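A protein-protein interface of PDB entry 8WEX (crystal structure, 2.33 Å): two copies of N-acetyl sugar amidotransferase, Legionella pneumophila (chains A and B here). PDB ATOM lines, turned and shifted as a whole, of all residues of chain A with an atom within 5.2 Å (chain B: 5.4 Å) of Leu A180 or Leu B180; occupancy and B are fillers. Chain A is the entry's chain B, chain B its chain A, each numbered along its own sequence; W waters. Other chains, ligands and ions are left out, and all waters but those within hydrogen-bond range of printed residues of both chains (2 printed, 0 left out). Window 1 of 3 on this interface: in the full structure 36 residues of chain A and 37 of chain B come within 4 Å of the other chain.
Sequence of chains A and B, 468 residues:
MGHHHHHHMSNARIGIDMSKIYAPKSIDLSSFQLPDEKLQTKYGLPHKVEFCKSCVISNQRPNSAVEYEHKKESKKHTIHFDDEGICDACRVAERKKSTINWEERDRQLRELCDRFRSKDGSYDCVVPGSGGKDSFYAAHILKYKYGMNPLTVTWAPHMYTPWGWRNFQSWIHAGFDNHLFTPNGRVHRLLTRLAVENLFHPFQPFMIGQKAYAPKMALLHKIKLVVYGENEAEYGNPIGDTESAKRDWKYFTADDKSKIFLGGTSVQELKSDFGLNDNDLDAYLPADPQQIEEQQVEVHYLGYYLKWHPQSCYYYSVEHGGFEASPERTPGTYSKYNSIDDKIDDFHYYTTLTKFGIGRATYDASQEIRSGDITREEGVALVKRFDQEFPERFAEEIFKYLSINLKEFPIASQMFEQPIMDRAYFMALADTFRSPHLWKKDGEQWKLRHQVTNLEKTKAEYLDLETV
N of Ala A156 sits at hydrogen-bond distance from O of Phe A181 (3.0 Å). O of Thr A154 is in hydrogen-bond range of N of Phe A181, 2.9 Å away. N of Phe A181 is in hydrogen-bond range of OH of Tyr A213. The side-chain hydroxyl of Tyr A213 sits at hydrogen-bond distance from the backbone carbonyl oxygen of His A179 (3.0 Å). The backbone carbonyl oxygen of Thr B154 is in hydrogen-bond range of the backbone NH of Phe B181, 2.8 Å away. N of Thr B154 sits at hydrogen-bond distance from O of His B179, at 2.9 Å.
Printed residues of chain B that touch a printed residue of chain A: Asn B178, His B179, Leu B180, Phe B181, Thr B182 and Tyr B213. Hydrophobic or aromatic side chains of chain B within 4 Å of the printed part of chain A: His B179, Leu B180, Phe B181 and Tyr B213. Of the 12 printed residues of chain A, 6 touch a printed residue of chain B. Along chain A the printed residues that touch a printed residue of chain B span positions 178 to 213. Among the printed residues, 14 pairs touch across the chains. Among the printed residues, no Asp or Glu carboxylate lies within 4 Å of a Lys or Arg side-chain nitrogen of the other chain.
Among the printed residues, merely in contact across the chains: Asn A178 with Leu B180, Asn A178 with Phe B181, His A179 with Leu B180, His A179 with Phe B181, Leu A180 with Asn B178, Leu A180 with His B179, Phe A181 with Asn B178 and Phe A181 with His B179.
Of chain B, only Asn B178, His B179 and Leu B180 come within 4 Å of Leu A180. Of the printed residues of chain A, Leu B180 touches Asn A178 (3.5 Å), His A179 (3.3 Å) and Leu A180 (2.7 Å). Of the printed residues of chain B, His A179 touches His B179, Leu B180, Phe B181 and Tyr B213. Of the printed residues of chain A, Tyr B213 touches His A179. Of the printed residues of chain A, Asn B178 touches Leu A180, Phe A181 and Thr A182. Of the printed residues of chain A, His B179 touches His A179 (3.2 Å), Leu A180 (3.3 Å), Phe A181 (3.8 Å) and Tyr A213 (2.9 Å). Of the printed residues of chain A, Thr B182 touches Asn A178. Thr A154 touches none of the printed residues of chain B. Phe B168 touches none of the printed residues of chain A.
NE2 of His A179 is in hydrogen-bond range of OH of Tyr B213 (3.0 Å). N of Leu A180 sits at hydrogen-bond distance from O of Leu B180, at 2.7 Å. ND1 of His B179 sits close to NE2 of His A179. The backbone carbonyl oxygen (O) of Asn B178 sits at hydrogen-bond distance from the backbone NH (N) of Thr A182 (2.8 Å). NE2 of His B179 sits at hydrogen-bond distance from OH of Tyr A213, at 2.9 Å. The backbone NH of Thr B182 sits at hydrogen-bond distance from the backbone carbonyl oxygen of Asn A178, at 2.8 Å.
Asn A178 touches Thr B182, and with the chains exchanged Thr A182 touches Asn B178. His A179 touches Leu B180, and with the chains exchanged Leu A180 touches His B179. His A179 touches Phe B181, and with the chains exchanged Phe A181 touches His B179. Leu B180 touches its own counterpart, Leu A180. Of the 14 pairs that touch across the chains among the printed residues, 14 have their exchanged pair printed and touching as well.
Water W1 lies within hydrogen-bond range of OG1 of Thr A182 (2.6 Å), OD1 of Asn B178 (2.8 Å) and O of Leu A180 (3.0 Å). Water W2 lies within hydrogen-bond range of OG1 of Thr B182 (2.6 Å), O of Leu B180 (2.8 Å) and OD1 of Asn A178 (2.9 Å).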
ATOM      1  N   THR A 154       3.463 -25.384   7.026  1.00  0.00           N
ATOM      2  CA  THR A 154       4.297 -25.413   5.813  1.00  0.00           C
ATOM      3  C   THR A 154       5.708 -24.967   6.178  1.00  0.00           C
ATOM      4  O   THR A 154       5.887 -23.834   6.683  1.00  0.00           O
ATOM      5  CB  THR A 154       3.698 -24.564   4.685  1.00  0.00           C
ATOM      6  OG1 THR A 154       2.329 -24.917   4.451  1.00  0.00           O
ATOM      7  CG2 THR A 154       4.466 -24.722   3.392  1.00  0.00           C
ATOM      8  N   TRP A 155       6.673 -25.854   5.946  1.00  0.00           N
ATOM      9  CA  TRP A 155       8.097 -25.478   5.844  1.00  0.00           C
ATOM     10  C   TRP A 155       8.262 -24.905   4.442  1.00  0.00           C
ATOM     11  O   TRP A 155       7.927 -25.593   3.495  1.00  0.00           O
ATOM     12  CB  TRP A 155       9.001 -26.685   6.102  1.00  0.00           C
ATOM     13  CG  TRP A 155      10.469 -26.389   6.063  1.00  0.00           C
ATOM     14  CD1 TRP A 155      11.326 -26.578   5.017  1.00  0.00           C
ATOM     15  CD2 TRP A 155      11.266 -25.877   7.145  1.00  0.00           C
ATOM     16  NE1 TRP A 155      12.593 -26.192   5.367  1.00  0.00           N
ATOM     17  CE2 TRP A 155      12.592 -25.783   6.672  1.00  0.00           C
ATOM     18  CE3 TRP A 155      10.994 -25.498   8.463  1.00  0.00           C
ATOM     19  CZ2 TRP A 155      13.629 -25.310   7.464  1.00  0.00           C
ATOM     20  CZ3 TRP A 155      12.025 -25.039   9.251  1.00  0.00           C
ATOM     21  CH2 TRP A 155      13.322 -24.940   8.752  1.00  0.00           C
ATOM     22  N   ALA A 156       8.686 -23.660   4.335  1.00  0.00           N
ATOM     23  CA  ALA A 156       8.603 -22.888   3.084  1.00  0.00           C
ATOM     24  C   ALA A 156       9.524 -23.512   2.049  1.00  0.00           C
ATOM     25  O   ALA A 156      10.613 -23.982   2.351  1.00  0.00           O
ATOM     26  CB  ALA A 156       8.963 -21.440   3.325  1.00  0.00           C
ATOM     27  N   PRO A 157       9.135 -23.464   0.767  1.00  0.00           N
ATOM     28  CA  PRO A 157      10.053 -23.855  -0.291  1.00  0.00           C
ATOM     29  C   PRO A 157      11.182 -22.818  -0.402  1.00  0.00           C
ATOM     30  O   PRO A 157      11.102 -21.742   0.165  1.00  0.00           O
ATOM     31  CB  PRO A 157       9.169 -23.859  -1.534  1.00  0.00           C
ATOM     32  CG  PRO A 157       8.109 -22.809  -1.223  1.00  0.00           C
ATOM     33  CD  PRO A 157       7.868 -22.917   0.267  1.00  0.00           C
ATOM     34  N   TYR A 160       9.125 -20.137  -4.388  1.00  0.00           N
ATOM     35  CA  TYR A 160       7.759 -20.469  -4.830  1.00  0.00           C
ATOM     36  C   TYR A 160       7.703 -20.347  -6.350  1.00  0.00           C
ATOM     37  O   TYR A 160       8.131 -19.317  -6.940  1.00  0.00           O
ATOM     38  CB  TYR A 160       6.718 -19.542  -4.186  1.00  0.00           C
ATOM     39  CG  TYR A 160       6.146 -20.069  -2.893  1.00  0.00           C
ATOM     40  CD1 TYR A 160       5.242 -21.114  -2.910  1.00  0.00           C
ATOM     41  CD2 TYR A 160       6.508 -19.545  -1.663  1.00  0.00           C
ATOM     42  CE1 TYR A 160       4.722 -21.640  -1.746  1.00  0.00           C
ATOM     43  CE2 TYR A 160       5.978 -20.043  -0.483  1.00  0.00           C
ATOM     44  CZ  TYR A 160       5.077 -21.096  -0.527  1.00  0.00           C
ATOM     45  OH  TYR A 160       4.554 -21.636   0.621  1.00  0.00           O
ATOM     46  N   PHE A 168      -0.886 -23.243  -2.665  1.00  0.00           N
ATOM     47  CA  PHE A 168      -0.780 -22.986  -1.210  1.00  0.00           C
ATOM     48  C   PHE A 168      -1.989 -22.146  -0.768  1.00  0.00           C
ATOM     49  O   PHE A 168      -2.645 -22.473   0.225  1.00  0.00           O
ATOM     50  CB  PHE A 168       0.567 -22.326  -0.931  1.00  0.00           C
ATOM     51  CG  PHE A 168       0.723 -21.768   0.449  1.00  0.00           C
ATOM     52  CD1 PHE A 168       0.840 -22.614   1.537  1.00  0.00           C
ATOM     53  CD2 PHE A 168       0.758 -20.400   0.657  1.00  0.00           C
ATOM     54  CE1 PHE A 168       0.985 -22.098   2.815  1.00  0.00           C
ATOM     55  CE2 PHE A 168       0.880 -19.891   1.938  1.00  0.00           C
ATOM     56  CZ  PHE A 168       1.008 -20.739   3.010  1.00  0.00           C
ATOM     57  N   ASN A 178      -3.198 -21.918   8.415  1.00  0.00           N
ATOM     58  CA  ASN A 178      -1.865 -22.380   7.989  1.00  0.00           C
ATOM     59  C   ASN A 178      -0.803 -21.582   8.708  1.00  0.00           C
ATOM     60  O   ASN A 178      -0.902 -20.343   8.731  1.00  0.00           O
ATOM     61  CB  ASN A 178      -1.647 -22.230   6.489  1.00  0.00           C
ATOM     62  CG  ASN A 178      -0.254 -22.658   6.100  1.00  0.00           C
ATOM     63  OD1 ASN A 178       0.642 -21.818   6.018  1.00  0.00           O
ATOM     64  ND2 ASN A 178      -0.080 -23.959   5.903  1.00  0.00           N
ATOM     65  N   HIS A 179       0.182 -22.279   9.259  1.00  0.00           N
ATOM     66  CA  HIS A 179       1.373 -21.647   9.852  1.00  0.00           C
ATOM     67  C   HIS A 179       2.547 -21.981   8.941  1.00  0.00           C
ATOM     68  O   HIS A 179       2.955 -23.158   8.892  1.00  0.00           O
ATOM     69  CB  HIS A 179       1.524 -22.046  11.325  1.00  0.00           C
ATOM     70  CG  HIS A 179       1.963 -20.920  12.202  1.00  0.00           C
ATOM     71  ND1 HIS A 179       1.947 -20.995  13.578  1.00  0.00           N
ATOM     72  CD2 HIS A 179       2.403 -19.681  11.900  1.00  0.00           C
ATOM     73  CE1 HIS A 179       2.403 -19.865  14.086  1.00  0.00           C
ATOM     74  NE2 HIS A 179       2.670 -19.038  13.076  1.00  0.00           N
ATOM     75  N   LEU A 180       3.035 -20.973   8.222  1.00  0.00           N
ATOM     76  CA  LEU A 180       4.173 -21.095   7.289  1.00  0.00           C
ATOM     77  C   LEU A 180       5.423 -20.553   7.985  1.00  0.00           C
ATOM     78  O   LEU A 180       5.449 -19.362   8.372  1.00  0.00           O
ATOM     79  CB  LEU A 180       3.880 -20.309   6.010  1.00  0.00           C
ATOM     80  CG  LEU A 180       5.070 -20.142   5.067  1.00  0.00           C
ATOM     81  CD1 LEU A 180       5.333 -21.434   4.318  1.00  0.00           C
ATOM     82  CD2 LEU A 180       4.848 -19.029   4.071  1.00  0.00           C
ATOM     83  N   PHE A 181       6.439 -21.397   8.111  1.00  0.00           N
ATOM     84  CA  PHE A 181       7.762 -20.976   8.604  1.00  0.00           C
ATOM     85  C   PHE A 181       8.680 -20.822   7.402  1.00  0.00           C
ATOM     86  O   PHE A 181       8.870 -21.794   6.634  1.00  0.00           O
ATOM     87  CB  PHE A 181       8.321 -21.970   9.615  1.00  0.00           C
ATOM     88  CG  PHE A 181       9.529 -21.431  10.324  1.00  0.00           C
ATOM     89  CD1 PHE A 181      10.794 -21.625   9.811  1.00  0.00           C
ATOM     90  CD2 PHE A 181       9.391 -20.700  11.493  1.00  0.00           C
ATOM     91  CE1 PHE A 181      11.903 -21.091  10.446  1.00  0.00           C
ATOM     92  CE2 PHE A 181      10.500 -20.184  12.135  1.00  0.00           C
ATOM     93  CZ  PHE A 181      11.759 -20.387  11.612  1.00  0.00           C
ATOM     94  N   THR A 182       9.217 -19.619   7.222  1.00  0.00           N
ATOM     95  CA  THR A 182      10.211 -19.355   6.163  1.00  0.00           C
ATOM     96  C   THR A 182      11.512 -19.040   6.872  1.00  0.00           C
ATOM     97  O   THR A 182      11.635 -18.001   7.524  1.00  0.00           O
ATOM     98  CB  THR A 182       9.798 -18.238   5.198  1.00  0.00           C
ATOM     99  OG1 THR A 182       8.463 -18.448   4.728  1.00  0.00           O
ATOM    100  CG2 THR A 182      10.732 -18.166   4.012  1.00  0.00           C
ATOM    101  N   TYR A 213      10.137 -29.901  11.272  1.00  0.00           N
ATOM    102  CA  TYR A 213       9.174 -28.774  11.420  1.00  0.00           C
ATOM    103  C   TYR A 213       7.863 -29.257  12.062  1.00  0.00           C
ATOM    104  O   TYR A 213       7.466 -28.711  13.110  1.00  0.00           O
ATOM    105  CB  TYR A 213       8.910 -28.096  10.080  1.00  0.00           C
ATOM    106  CG  TYR A 213       7.988 -26.909  10.175  1.00  0.00           C
ATOM    107  CD1 TYR A 213       8.254 -25.877  11.061  1.00  0.00           C
ATOM    108  CD2 TYR A 213       6.854 -26.814   9.378  1.00  0.00           C
ATOM    109  CE1 TYR A 213       7.397 -24.795  11.176  1.00  0.00           C
ATOM    110  CE2 TYR A 213       5.997 -25.732   9.468  1.00  0.00           C
ATOM    111  CZ  TYR A 213       6.268 -24.720  10.374  1.00  0.00           C
ATOM    112  OH  TYR A 213       5.441 -23.636  10.447  1.00  0.00           O
ATOM    113  N   THR B 154       4.053 -12.692  10.940  1.00  0.00           N
ATOM    114  CA  THR B 154       3.136 -12.040   9.978  1.00  0.00           C
ATOM    115  C   THR B 154       1.752 -12.653  10.108  1.00  0.00           C
ATOM    116  O   THR B 154       1.615 -13.868   9.892  1.00  0.00           O
ATOM    117  CB  THR B 154       3.630 -12.137   8.529  1.00  0.00           C
ATOM    118  OG1 THR B 154       4.962 -11.648   8.417  1.00  0.00           O
ATOM    119  CG2 THR B 154       2.782 -11.321   7.583  1.00  0.00           C
ATOM    120  N   TRP B 155       0.782 -11.827  10.488  1.00  0.00           N
ATOM    121  CA  TRP B 155      -0.654 -12.111  10.276  1.00  0.00           C
ATOM    122  C   TRP B 155      -0.930 -11.821   8.810  1.00  0.00           C
ATOM    123  O   TRP B 155      -0.638 -10.705   8.376  1.00  0.00           O
ATOM    124  CB  TRP B 155      -1.504 -11.246  11.207  1.00  0.00           C
ATOM    125  CG  TRP B 155      -2.968 -11.525  11.152  1.00  0.00           C
ATOM    126  CD1 TRP B 155      -3.906 -10.785  10.497  1.00  0.00           C
ATOM    127  CD2 TRP B 155      -3.675 -12.578  11.828  1.00  0.00           C
ATOM    128  NE1 TRP B 155      -5.156 -11.308  10.717  1.00  0.00           N
ATOM    129  CE2 TRP B 155      -5.038 -12.430  11.499  1.00  0.00           C
ATOM    130  CE3 TRP B 155      -3.295 -13.620  12.678  1.00  0.00           C
ATOM    131  CZ2 TRP B 155      -6.013 -13.287  11.993  1.00  0.00           C
ATOM    132  CZ3 TRP B 155      -4.261 -14.482  13.152  1.00  0.00           C
ATOM    133  CH2 TRP B 155      -5.603 -14.305  12.823  1.00  0.00           C
ATOM    134  N   ALA B 156      -1.375 -12.818   8.059  1.00  0.00           N
ATOM    135  CA  ALA B 156      -1.413 -12.733   6.586  1.00  0.00           C
ATOM    136  C   ALA B 156      -2.409 -11.664   6.162  1.00  0.00           C
ATOM    137  O   ALA B 156      -3.470 -11.493   6.760  1.00  0.00           O
ATOM    138  CB  ALA B 156      -1.778 -14.064   5.972  1.00  0.00           C
ATOM    139  N   PRO B 157      -2.128 -10.954   5.062  1.00  0.00           N
ATOM    140  CA  PRO B 157      -3.110 -10.056   4.480  1.00  0.00           C
ATOM    141  C   PRO B 157      -4.264 -10.867   3.883  1.00  0.00           C
ATOM    142  O   PRO B 157      -4.159 -12.080   3.741  1.00  0.00           O
ATOM    143  CB  PRO B 157      -2.334  -9.299   3.402  1.00  0.00           C
ATOM    144  CG  PRO B 157      -1.202 -10.231   3.042  1.00  0.00           C
ATOM    145  CD  PRO B 157      -0.862 -10.980   4.317  1.00  0.00           C
ATOM    146  N   TYR B 160      -2.598 -10.850  -1.085  1.00  0.00           N
ATOM    147  CA  TYR B 160      -1.261 -10.294  -1.364  1.00  0.00           C
ATOM    148  C   TYR B 160      -1.325  -9.533  -2.684  1.00  0.00           C
ATOM    149  O   TYR B 160      -1.830 -10.071  -3.702  1.00  0.00           O
ATOM    150  CB  TYR B 160      -0.202 -11.394  -1.416  1.00  0.00           C
ATOM    151  CG  TYR B 160       0.479 -11.650  -0.095  1.00  0.00           C
ATOM    152  CD1 TYR B 160       1.380 -10.733   0.413  1.00  0.00           C
ATOM    153  CD2 TYR B 160       0.226 -12.789   0.650  1.00  0.00           C
ATOM    154  CE1 TYR B 160       2.017 -10.933   1.626  1.00  0.00           C
ATOM    155  CE2 TYR B 160       0.858 -13.007   1.869  1.00  0.00           C
ATOM    156  CZ  TYR B 160       1.765 -12.077   2.359  1.00  0.00           C
ATOM    157  OH  TYR B 160       2.414 -12.244   3.557  1.00  0.00           O
ATOM    158  N   PHE B 168       7.583  -8.986   1.302  1.00  0.00           N
ATOM    159  CA  PHE B 168       7.561  -9.967   2.410  1.00  0.00           C
ATOM    160  C   PHE B 168       8.774 -10.900   2.233  1.00  0.00           C
ATOM    161  O   PHE B 168       9.507 -11.209   3.199  1.00  0.00           O
ATOM    162  CB  PHE B 168       6.226 -10.703   2.398  1.00  0.00           C
ATOM    163  CG  PHE B 168       6.183 -11.936   3.262  1.00  0.00           C
ATOM    164  CD1 PHE B 168       6.209 -11.844   4.646  1.00  0.00           C
ATOM    165  CD2 PHE B 168       6.087 -13.190   2.684  1.00  0.00           C
ATOM    166  CE1 PHE B 168       6.202 -12.986   5.430  1.00  0.00           C
ATOM    167  CE2 PHE B 168       6.054 -14.326   3.473  1.00  0.00           C
ATOM    168  CZ  PHE B 168       6.112 -14.222   4.847  1.00  0.00           C
ATOM    169  N   ASN B 178      10.740 -16.203   9.614  1.00  0.00           N
ATOM    170  CA  ASN B 178       9.401 -15.588   9.626  1.00  0.00           C
ATOM    171  C   ASN B 178       8.381 -16.680   9.872  1.00  0.00           C
ATOM    172  O   ASN B 178       8.458 -17.733   9.201  1.00  0.00           O
ATOM    173  CB  ASN B 178       9.060 -14.858   8.340  1.00  0.00           C
ATOM    174  CG  ASN B 178       7.629 -14.358   8.375  1.00  0.00           C
ATOM    175  OD1 ASN B 178       6.710 -15.045   7.933  1.00  0.00           O
ATOM    176  ND2 ASN B 178       7.431 -13.182   8.939  1.00  0.00           N
ATOM    177  N   HIS B 179       7.477 -16.433  10.814  1.00  0.00           N
ATOM    178  CA  HIS B 179       6.309 -17.309  11.019  1.00  0.00           C
ATOM    179  C   HIS B 179       5.065 -16.560  10.526  1.00  0.00           C
ATOM    180  O   HIS B 179       4.692 -15.524  11.112  1.00  0.00           O
ATOM    181  CB  HIS B 179       6.281 -17.785  12.457  1.00  0.00           C
ATOM    182  CG  HIS B 179       5.950 -19.236  12.559  1.00  0.00           C
ATOM    183  ND1 HIS B 179       5.948 -19.905  13.758  1.00  0.00           N
ATOM    184  CD2 HIS B 179       5.605 -20.142  11.619  1.00  0.00           C
ATOM    185  CE1 HIS B 179       5.585 -21.155  13.560  1.00  0.00           C
ATOM    186  NE2 HIS B 179       5.379 -21.325  12.256  1.00  0.00           N
ATOM    187  N   LEU B 180       4.521 -17.013   9.400  1.00  0.00           N
ATOM    188  CA  LEU B 180       3.321 -16.431   8.760  1.00  0.00           C
ATOM    189  C   LEU B 180       2.115 -17.290   9.126  1.00  0.00           C
ATOM    190  O   LEU B 180       2.106 -18.498   8.840  1.00  0.00           O
ATOM    191  CB  LEU B 180       3.520 -16.379   7.249  1.00  0.00           C
ATOM    192  CG  LEU B 180       2.284 -16.061   6.409  1.00  0.00           C
ATOM    193  CD1 LEU B 180       1.921 -14.580   6.495  1.00  0.00           C
ATOM    194  CD2 LEU B 180       2.529 -16.435   4.955  1.00  0.00           C
ATOM    195  N   PHE B 181       1.124 -16.670   9.751  1.00  0.00           N
ATOM    196  CA  PHE B 181      -0.178 -17.308  10.009  1.00  0.00           C
ATOM    197  C   PHE B 181      -1.153 -16.811   8.950  1.00  0.00           C
ATOM    198  O   PHE B 181      -1.361 -15.606   8.838  1.00  0.00           O
ATOM    199  CB  PHE B 181      -0.663 -17.031  11.429  1.00  0.00           C
ATOM    200  CG  PHE B 181      -1.893 -17.830  11.765  1.00  0.00           C
ATOM    201  CD1 PHE B 181      -1.785 -19.086  12.333  1.00  0.00           C
ATOM    202  CD2 PHE B 181      -3.149 -17.363  11.411  1.00  0.00           C
ATOM    203  CE1 PHE B 181      -2.918 -19.837  12.602  1.00  0.00           C
ATOM    204  CE2 PHE B 181      -4.278 -18.117  11.675  1.00  0.00           C
ATOM    205  CZ  PHE B 181      -4.160 -19.344  12.284  1.00  0.00           C
ATOM    206  N   THR B 182      -1.729 -17.723   8.175  1.00  0.00           N
ATOM    207  CA  THR B 182      -2.808 -17.386   7.220  1.00  0.00           C
ATOM    208  C   THR B 182      -4.062 -18.067   7.725  1.00  0.00           C
ATOM    209  O   THR B 182      -4.141 -19.291   7.715  1.00  0.00           O
ATOM    210  CB  THR B 182      -2.488 -17.787   5.779  1.00  0.00           C
ATOM    211  OG1 THR B 182      -1.182 -17.341   5.404  1.00  0.00           O
ATOM    212  CG2 THR B 182      -3.508 -17.219   4.817  1.00  0.00           C
ATOM    213  N   TYR B 213      -2.256 -11.459  17.440  1.00  0.00           N
ATOM    214  CA  TYR B 213      -1.290 -12.434  16.872  1.00  0.00           C
ATOM    215  C   TYR B 213       0.063 -12.375  17.586  1.00  0.00           C
ATOM    216  O   TYR B 213       0.546 -13.408  18.091  1.00  0.00           O
ATOM    217  CB  TYR B 213      -1.113 -12.236  15.369  1.00  0.00           C
ATOM    218  CG  TYR B 213      -0.245 -13.289  14.728  1.00  0.00           C
ATOM    219  CD1 TYR B 213      -0.450 -14.641  14.968  1.00  0.00           C
ATOM    220  CD2 TYR B 213       0.763 -12.931  13.853  1.00  0.00           C
ATOM    221  CE1 TYR B 213       0.339 -15.608  14.370  1.00  0.00           C
ATOM    222  CE2 TYR B 213       1.561 -13.885  13.242  1.00  0.00           C
ATOM    223  CZ  TYR B 213       1.344 -15.225  13.498  1.00  0.00           C
ATOM    224  OH  TYR B 213       2.144 -16.141  12.890  1.00  0.00           O
HETATM  225  O   HOH W   1       6.832 -17.469   6.486  1.00  0.00           O
HETATM  226  O   HOH W   2       0.587 -18.937   6.499  1.00  0.00           O
